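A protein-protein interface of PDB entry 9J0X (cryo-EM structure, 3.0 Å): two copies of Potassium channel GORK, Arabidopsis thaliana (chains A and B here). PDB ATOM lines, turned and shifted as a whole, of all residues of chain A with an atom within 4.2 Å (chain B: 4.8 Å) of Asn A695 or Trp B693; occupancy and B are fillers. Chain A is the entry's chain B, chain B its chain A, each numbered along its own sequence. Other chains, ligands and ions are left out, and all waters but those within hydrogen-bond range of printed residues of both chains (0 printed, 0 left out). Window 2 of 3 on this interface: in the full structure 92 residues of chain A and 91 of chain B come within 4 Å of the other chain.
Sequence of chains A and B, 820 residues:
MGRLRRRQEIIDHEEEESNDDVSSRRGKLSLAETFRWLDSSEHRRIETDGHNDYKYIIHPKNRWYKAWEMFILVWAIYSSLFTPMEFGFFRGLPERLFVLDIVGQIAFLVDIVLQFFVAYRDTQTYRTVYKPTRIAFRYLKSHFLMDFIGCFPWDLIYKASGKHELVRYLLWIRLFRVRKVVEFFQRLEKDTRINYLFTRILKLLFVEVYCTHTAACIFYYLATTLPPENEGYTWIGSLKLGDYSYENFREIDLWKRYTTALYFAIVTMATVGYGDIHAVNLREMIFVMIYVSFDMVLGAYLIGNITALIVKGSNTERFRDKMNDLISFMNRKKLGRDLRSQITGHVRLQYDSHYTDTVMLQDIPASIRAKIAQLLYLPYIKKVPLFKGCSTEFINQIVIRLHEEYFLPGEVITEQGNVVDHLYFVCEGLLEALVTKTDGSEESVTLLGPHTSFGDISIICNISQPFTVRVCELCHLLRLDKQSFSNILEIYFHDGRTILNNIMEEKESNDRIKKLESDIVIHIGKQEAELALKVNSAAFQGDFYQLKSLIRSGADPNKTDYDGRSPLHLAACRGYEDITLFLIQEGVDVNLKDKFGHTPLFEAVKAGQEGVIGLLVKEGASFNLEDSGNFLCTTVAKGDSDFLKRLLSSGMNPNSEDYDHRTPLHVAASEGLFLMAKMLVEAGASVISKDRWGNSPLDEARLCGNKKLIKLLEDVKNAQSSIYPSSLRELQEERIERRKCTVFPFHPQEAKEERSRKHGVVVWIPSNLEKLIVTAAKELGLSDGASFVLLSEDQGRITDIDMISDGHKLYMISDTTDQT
NH1 of Arg A662 sits close to NE1 of Trp B693, at 3.3 Å.
OD1 of Asn B695 sits at hydrogen-bond distance from NE1 of Trp A693, 3.0 Å away.
The guanidinium group of Arg B692 lies within salt-bridge range of the side-chain carboxylate of Glu A700.
NH1 of Arg A662 sits close to NH2 of Arg B692 (3.3 Å).
OD1 of Asn A695 sits close to OD2 of Asp A699.
The side-chain carboxylate (OD1) of Asp A691 is in hydrogen-bond range of the backbone NH (N) of Asn A695 (2.5 Å).
OD1 of Asp A691 sits at hydrogen-bond distance from N of Gly A694, at 2.9 Å.
The backbone NH of Trp A693 sits close to the side-chain carboxylate of Asp A691, 3.3 Å away.
O of Trp A693 lies within hydrogen-bond range of ND2 of Asn A695 (3.2 Å).
The backbone carbonyl oxygen (O) of His A666 lies within hydrogen-bond range of the guanidinium group (NH2) of Arg A662.
NE2 of His A666 touches CH2 of Trp B693 (3.3 Å).
Asp A691 touches Trp B693 (OD2 to CZ2, 3.2 Å).
CZ2 of Trp A693 touches OD2 of Asp B691 (3.3 Å).
Trp A693 touches Trp B693 (CZ3 to NE1, 3.5 Å).
ND2 of Asn A695 touches CZ3 of Trp B693, at 3.5 Å.
Trp B693 touches Glu A700.
Of chain B, only Trp B693 comes within 4 Å of Asn A695.
Trp B693 touches just these residues of chain A: Arg A662, His A666, Asp A691, Trp A693, Asn A695 and Glu A700.
Printed residues of chain A within 4 Å of Arg B692: Arg A662 (3.3 Å) and Glu A700 (2.8 Å).
Printed residues of chain A within 4 Å of Asn B695: Trp A693 (3.0 Å).
Gly B694 touches none of the printed residues of chain A.
Gly A694 touches none of the printed residues of chain B.
The nearest printed residue of chain B that does not touch Asn A695 is Arg B692 (7.6 Å).
The nearest printed residue of chain B that does not touch Asp A691 is Arg B692 (6.6 Å).
Of the 5 printed residues of chain B, 4 touch a printed residue of chain A.
Hydrophobic or aromatic side chains of chain B within 4 Å of the printed part of chain A: Trp B693.
Printed residues of chain A that touch a printed residue of chain B: Arg A662, His A666, Asp A691, Trp A693, Asn A695 and Glu A700.
Hydrophobic or aromatic side chains of chain A within 4 Å of the printed part of chain B: His A666 and Trp A693.
Among the printed residues, Asp or Glu carboxylates within 4 Å of a Lys or Arg side-chain nitrogen of the other chain: Glu A700 with Arg B692 (2.8 Å).
Asp A691 touches Trp B693, and with the chains exchanged Trp A693 touches Asp B691.
Trp A693 touches its own counterpart, Trp B693.
Trp A693 touches Asn B695, and with the chains exchanged Asn A695 touches Trp B693.
Positions printed for both chains: 691, 693, 694 and 695.
Of the 10 pairs that touch across the chains among the printed residues, 5 have their exchanged pair printed and touching as well.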
ATOM      1  N   ARG A 662     -30.559 -14.165  11.295  1.00  0.00           N
ATOM      2  CA  ARG A 662     -31.325 -14.086  12.531  1.00  0.00           C
ATOM      3  C   ARG A 662     -32.394 -15.170  12.524  1.00  0.00           C
ATOM      4  O   ARG A 662     -33.237 -15.210  11.621  1.00  0.00           O
ATOM      5  CB  ARG A 662     -31.964 -12.707  12.698  1.00  0.00           C
ATOM      6  CG  ARG A 662     -30.971 -11.612  13.018  1.00  0.00           C
ATOM      7  CD  ARG A 662     -31.643 -10.262  13.190  1.00  0.00           C
ATOM      8  NE  ARG A 662     -32.876 -10.346  13.965  1.00  0.00           N
ATOM      9  CZ  ARG A 662     -33.378  -9.339  14.672  1.00  0.00           C
ATOM     10  NH1 ARG A 662     -32.746  -8.175  14.708  1.00  0.00           N
ATOM     11  NH2 ARG A 662     -34.507  -9.497  15.347  1.00  0.00           N
ATOM     12  N   HIS A 666     -34.727 -14.980  17.403  1.00  0.00           N
ATOM     13  CA  HIS A 666     -34.058 -13.691  17.535  1.00  0.00           C
ATOM     14  C   HIS A 666     -34.992 -12.523  17.252  1.00  0.00           C
ATOM     15  O   HIS A 666     -34.702 -11.401  17.676  1.00  0.00           O
ATOM     16  CB  HIS A 666     -32.852 -13.626  16.599  1.00  0.00           C
ATOM     17  CG  HIS A 666     -31.763 -12.720  17.075  1.00  0.00           C
ATOM     18  ND1 HIS A 666     -30.929 -13.048  18.121  1.00  0.00           N
ATOM     19  CD2 HIS A 666     -31.363 -11.501  16.643  1.00  0.00           C
ATOM     20  CE1 HIS A 666     -30.065 -12.068  18.317  1.00  0.00           C
ATOM     21  NE2 HIS A 666     -30.306 -11.119  17.431  1.00  0.00           N
ATOM     22  N   SER A 689     -26.950 -19.093  18.657  1.00  0.00           N
ATOM     23  CA  SER A 689     -26.695 -18.839  17.240  1.00  0.00           C
ATOM     24  C   SER A 689     -26.716 -17.331  17.054  1.00  0.00           C
ATOM     25  O   SER A 689     -27.708 -16.683  17.403  1.00  0.00           O
ATOM     26  CB  SER A 689     -27.738 -19.513  16.351  1.00  0.00           C
ATOM     27  OG  SER A 689     -29.015 -18.932  16.532  1.00  0.00           O
ATOM     28  N   LYS A 690     -25.641 -16.774  16.508  1.00  0.00           N
ATOM     29  CA  LYS A 690     -25.425 -15.334  16.537  1.00  0.00           C
ATOM     30  C   LYS A 690     -26.104 -14.659  15.344  1.00  0.00           C
ATOM     31  O   LYS A 690     -26.880 -15.271  14.606  1.00  0.00           O
ATOM     32  CB  LYS A 690     -23.928 -15.030  16.584  1.00  0.00           C
ATOM     33  CG  LYS A 690     -23.374 -14.837  17.990  1.00  0.00           C
ATOM     34  CD  LYS A 690     -23.218 -16.159  18.727  1.00  0.00           C
ATOM     35  CE  LYS A 690     -22.933 -15.944  20.202  1.00  0.00           C
ATOM     36  NZ  LYS A 690     -22.891 -17.233  20.946  1.00  0.00           N
ATOM     37  N   ASP A 691     -25.814 -13.374  15.151  1.00  0.00           N
ATOM     38  CA  ASP A 691     -26.430 -12.569  14.104  1.00  0.00           C
ATOM     39  C   ASP A 691     -25.374 -11.618  13.547  1.00  0.00           C
ATOM     40  O   ASP A 691     -24.172 -11.808  13.754  1.00  0.00           O
ATOM     41  CB  ASP A 691     -27.665 -11.837  14.646  1.00  0.00           C
ATOM     42  CG  ASP A 691     -27.309 -10.714  15.599  1.00  0.00           C
ATOM     43  OD1 ASP A 691     -26.401 -10.905  16.430  1.00  0.00           O
ATOM     44  OD2 ASP A 691     -27.931  -9.635  15.507  1.00  0.00           O
ATOM     45  N   TRP A 693     -25.004  -8.561  14.510  1.00  0.00           N
ATOM     46  CA  TRP A 693     -24.464  -7.844  15.656  1.00  0.00           C
ATOM     47  C   TRP A 693     -23.725  -8.753  16.628  1.00  0.00           C
ATOM     48  O   TRP A 693     -23.206  -8.264  17.637  1.00  0.00           O
ATOM     49  CB  TRP A 693     -25.583  -7.111  16.399  1.00  0.00           C
ATOM     50  CG  TRP A 693     -26.029  -5.852  15.737  1.00  0.00           C
ATOM     51  CD1 TRP A 693     -25.664  -4.579  16.065  1.00  0.00           C
ATOM     52  CD2 TRP A 693     -26.934  -5.737  14.634  1.00  0.00           C
ATOM     53  NE1 TRP A 693     -26.282  -3.679  15.232  1.00  0.00           N
ATOM     54  CE2 TRP A 693     -27.068  -4.365  14.345  1.00  0.00           C
ATOM     55  CE3 TRP A 693     -27.643  -6.662  13.862  1.00  0.00           C
ATOM     56  CZ2 TRP A 693     -27.880  -3.896  13.316  1.00  0.00           C
ATOM     57  CZ3 TRP A 693     -28.450  -6.194  12.842  1.00  0.00           C
ATOM     58  CH2 TRP A 693     -28.561  -4.824  12.579  1.00  0.00           C
ATOM     59  N   GLY A 694     -23.661 -10.053  16.353  1.00  0.00           N
ATOM     60  CA  GLY A 694     -23.004 -10.976  17.254  1.00  0.00           C
ATOM     61  C   GLY A 694     -23.784 -11.312  18.502  1.00  0.00           C
ATOM     62  O   GLY A 694     -23.202 -11.820  19.465  1.00  0.00           O
ATOM     63  N   ASN A 695     -25.085 -11.037  18.521  1.00  0.00           N
ATOM     64  CA  ASN A 695     -25.923 -11.337  19.673  1.00  0.00           C
ATOM     65  C   ASN A 695     -26.627 -12.673  19.485  1.00  0.00           C
ATOM     66  O   ASN A 695     -27.067 -13.011  18.382  1.00  0.00           O
ATOM     67  CB  ASN A 695     -26.960 -10.235  19.892  1.00  0.00           C
ATOM     68  CG  ASN A 695     -26.358  -8.977  20.478  1.00  0.00           C
ATOM     69  OD1 ASN A 695     -26.423  -8.748  21.685  1.00  0.00           O
ATOM     70  ND2 ASN A 695     -25.767  -8.152  19.624  1.00  0.00           N
ATOM     71  N   SER A 696     -26.718 -13.425  20.559  1.00  0.00           N
ATOM     72  CA  SER A 696     -27.551 -14.612  20.630  1.00  0.00           C
ATOM     73  C   SER A 696     -28.970 -14.202  21.006  1.00  0.00           C
ATOM     74  O   SER A 696     -29.198 -13.076  21.450  1.00  0.00           O
ATOM     75  CB  SER A 696     -26.967 -15.590  21.658  1.00  0.00           C
ATOM     76  OG  SER A 696     -27.832 -16.673  21.962  1.00  0.00           O
ATOM     77  N   ASP A 699     -29.259 -12.878  25.173  1.00  0.00           N
ATOM     78  CA  ASP A 699     -29.222 -11.474  25.558  1.00  0.00           C
ATOM     79  C   ASP A 699     -30.060 -10.586  24.648  1.00  0.00           C
ATOM     80  O   ASP A 699     -30.246  -9.406  24.965  1.00  0.00           O
ATOM     81  CB  ASP A 699     -27.773 -10.976  25.619  1.00  0.00           C
ATOM     82  CG  ASP A 699     -27.005 -11.219  24.337  1.00  0.00           C
ATOM     83  OD1 ASP A 699     -27.535 -11.887  23.429  1.00  0.00           O
ATOM     84  OD2 ASP A 699     -25.859 -10.731  24.231  1.00  0.00           O
ATOM     85  N   GLU A 700     -30.551 -11.113  23.525  1.00  0.00           N
ATOM     86  CA  GLU A 700     -31.578 -10.401  22.774  1.00  0.00           C
ATOM     87  C   GLU A 700     -32.895 -10.397  23.539  1.00  0.00           C
ATOM     88  O   GLU A 700     -33.622  -9.397  23.538  1.00  0.00           O
ATOM     89  CB  GLU A 700     -31.746 -11.031  21.389  1.00  0.00           C
ATOM     90  CG  GLU A 700     -32.846 -10.433  20.520  1.00  0.00           C
ATOM     91  CD  GLU A 700     -32.830  -8.917  20.495  1.00  0.00           C
ATOM     92  OE1 GLU A 700     -31.766  -8.325  20.224  1.00  0.00           O
ATOM     93  OE2 GLU A 700     -33.892  -8.314  20.749  1.00  0.00           O
ATOM     94  N   ASP B 691     -31.752   1.698  14.162  1.00  0.00           N
ATOM     95  CA  ASP B 691     -32.373   0.386  14.080  1.00  0.00           C
ATOM     96  C   ASP B 691     -33.265   0.160  15.298  1.00  0.00           C
ATOM     97  O   ASP B 691     -33.496   1.056  16.114  1.00  0.00           O
ATOM     98  CB  ASP B 691     -31.305  -0.698  13.983  1.00  0.00           C
ATOM     99  CG  ASP B 691     -30.460  -0.572  12.741  1.00  0.00           C
ATOM    100  OD1 ASP B 691     -30.957  -0.031  11.733  1.00  0.00           O
ATOM    101  OD2 ASP B 691     -29.294  -1.013  12.776  1.00  0.00           O
ATOM    102  N   ARG B 692     -33.783  -1.063  15.427  1.00  0.00           N
ATOM    103  CA  ARG B 692     -34.260  -1.519  16.724  1.00  0.00           C
ATOM    104  C   ARG B 692     -33.101  -1.651  17.701  1.00  0.00           C
ATOM    105  O   ARG B 692     -33.275  -1.434  18.906  1.00  0.00           O
ATOM    106  CB  ARG B 692     -34.997  -2.850  16.573  1.00  0.00           C
ATOM    107  CG  ARG B 692     -35.965  -3.160  17.700  1.00  0.00           C
ATOM    108  CD  ARG B 692     -35.364  -4.158  18.673  1.00  0.00           C
ATOM    109  NE  ARG B 692     -34.939  -5.384  18.004  1.00  0.00           N
ATOM    110  CZ  ARG B 692     -33.961  -6.171  18.443  1.00  0.00           C
ATOM    111  NH1 ARG B 692     -33.308  -5.859  19.553  1.00  0.00           N
ATOM    112  NH2 ARG B 692     -33.643  -7.272  17.775  1.00  0.00           N
ATOM    113  N   TRP B 693     -31.917  -1.996  17.194  1.00  0.00           N
ATOM    114  CA  TRP B 693     -30.695  -1.942  17.985  1.00  0.00           C
ATOM    115  C   TRP B 693     -30.258  -0.512  18.270  1.00  0.00           C
ATOM    116  O   TRP B 693     -29.530  -0.282  19.241  1.00  0.00           O
ATOM    117  CB  TRP B 693     -29.566  -2.685  17.267  1.00  0.00           C
ATOM    118  CG  TRP B 693     -29.940  -4.032  16.731  1.00  0.00           C
ATOM    119  CD1 TRP B 693     -30.559  -4.306  15.543  1.00  0.00           C
ATOM    120  CD2 TRP B 693     -29.689  -5.295  17.351  1.00  0.00           C
ATOM    121  NE1 TRP B 693     -30.725  -5.659  15.397  1.00  0.00           N
ATOM    122  CE2 TRP B 693     -30.197  -6.291  16.492  1.00  0.00           C
ATOM    123  CE3 TRP B 693     -29.089  -5.683  18.554  1.00  0.00           C
ATOM    124  CZ2 TRP B 693     -30.123  -7.647  16.797  1.00  0.00           C
ATOM    125  CZ3 TRP B 693     -29.018  -7.030  18.854  1.00  0.00           C
ATOM    126  CH2 TRP B 693     -29.528  -7.994  17.979  1.00  0.00           C
ATOM    127  N   GLY B 694     -30.685   0.448  17.452  1.00  0.00           N
ATOM    128  CA  GLY B 694     -30.277   1.829  17.620  1.00  0.00           C
ATOM    129  C   GLY B 694     -28.980   2.161  16.911  1.00  0.00           C
ATOM    130  O   GLY B 694     -28.023   2.621  17.540  1.00  0.00           O
ATOM    131  N   ASN B 695     -28.936   1.934  15.599  1.00  0.00           N
ATOM    132  CA  ASN B 695     -27.719   2.128  14.822  1.00  0.00           C
ATOM    133  C   ASN B 695     -28.033   2.834  13.512  1.00  0.00           C
ATOM    134  O   ASN B 695     -28.806   2.325  12.696  1.00  0.00           O
ATOM    135  CB  ASN B 695     -27.028   0.791  14.531  1.00  0.00           C
ATOM    136  CG  ASN B 695     -26.495   0.126  15.783  1.00  0.00           C
ATOM    137  OD1 ASN B 695     -26.959  -0.944  16.177  1.00  0.00           O
ATOM    138  ND2 ASN B 695     -25.509   0.753  16.410  1.00  0.00           N
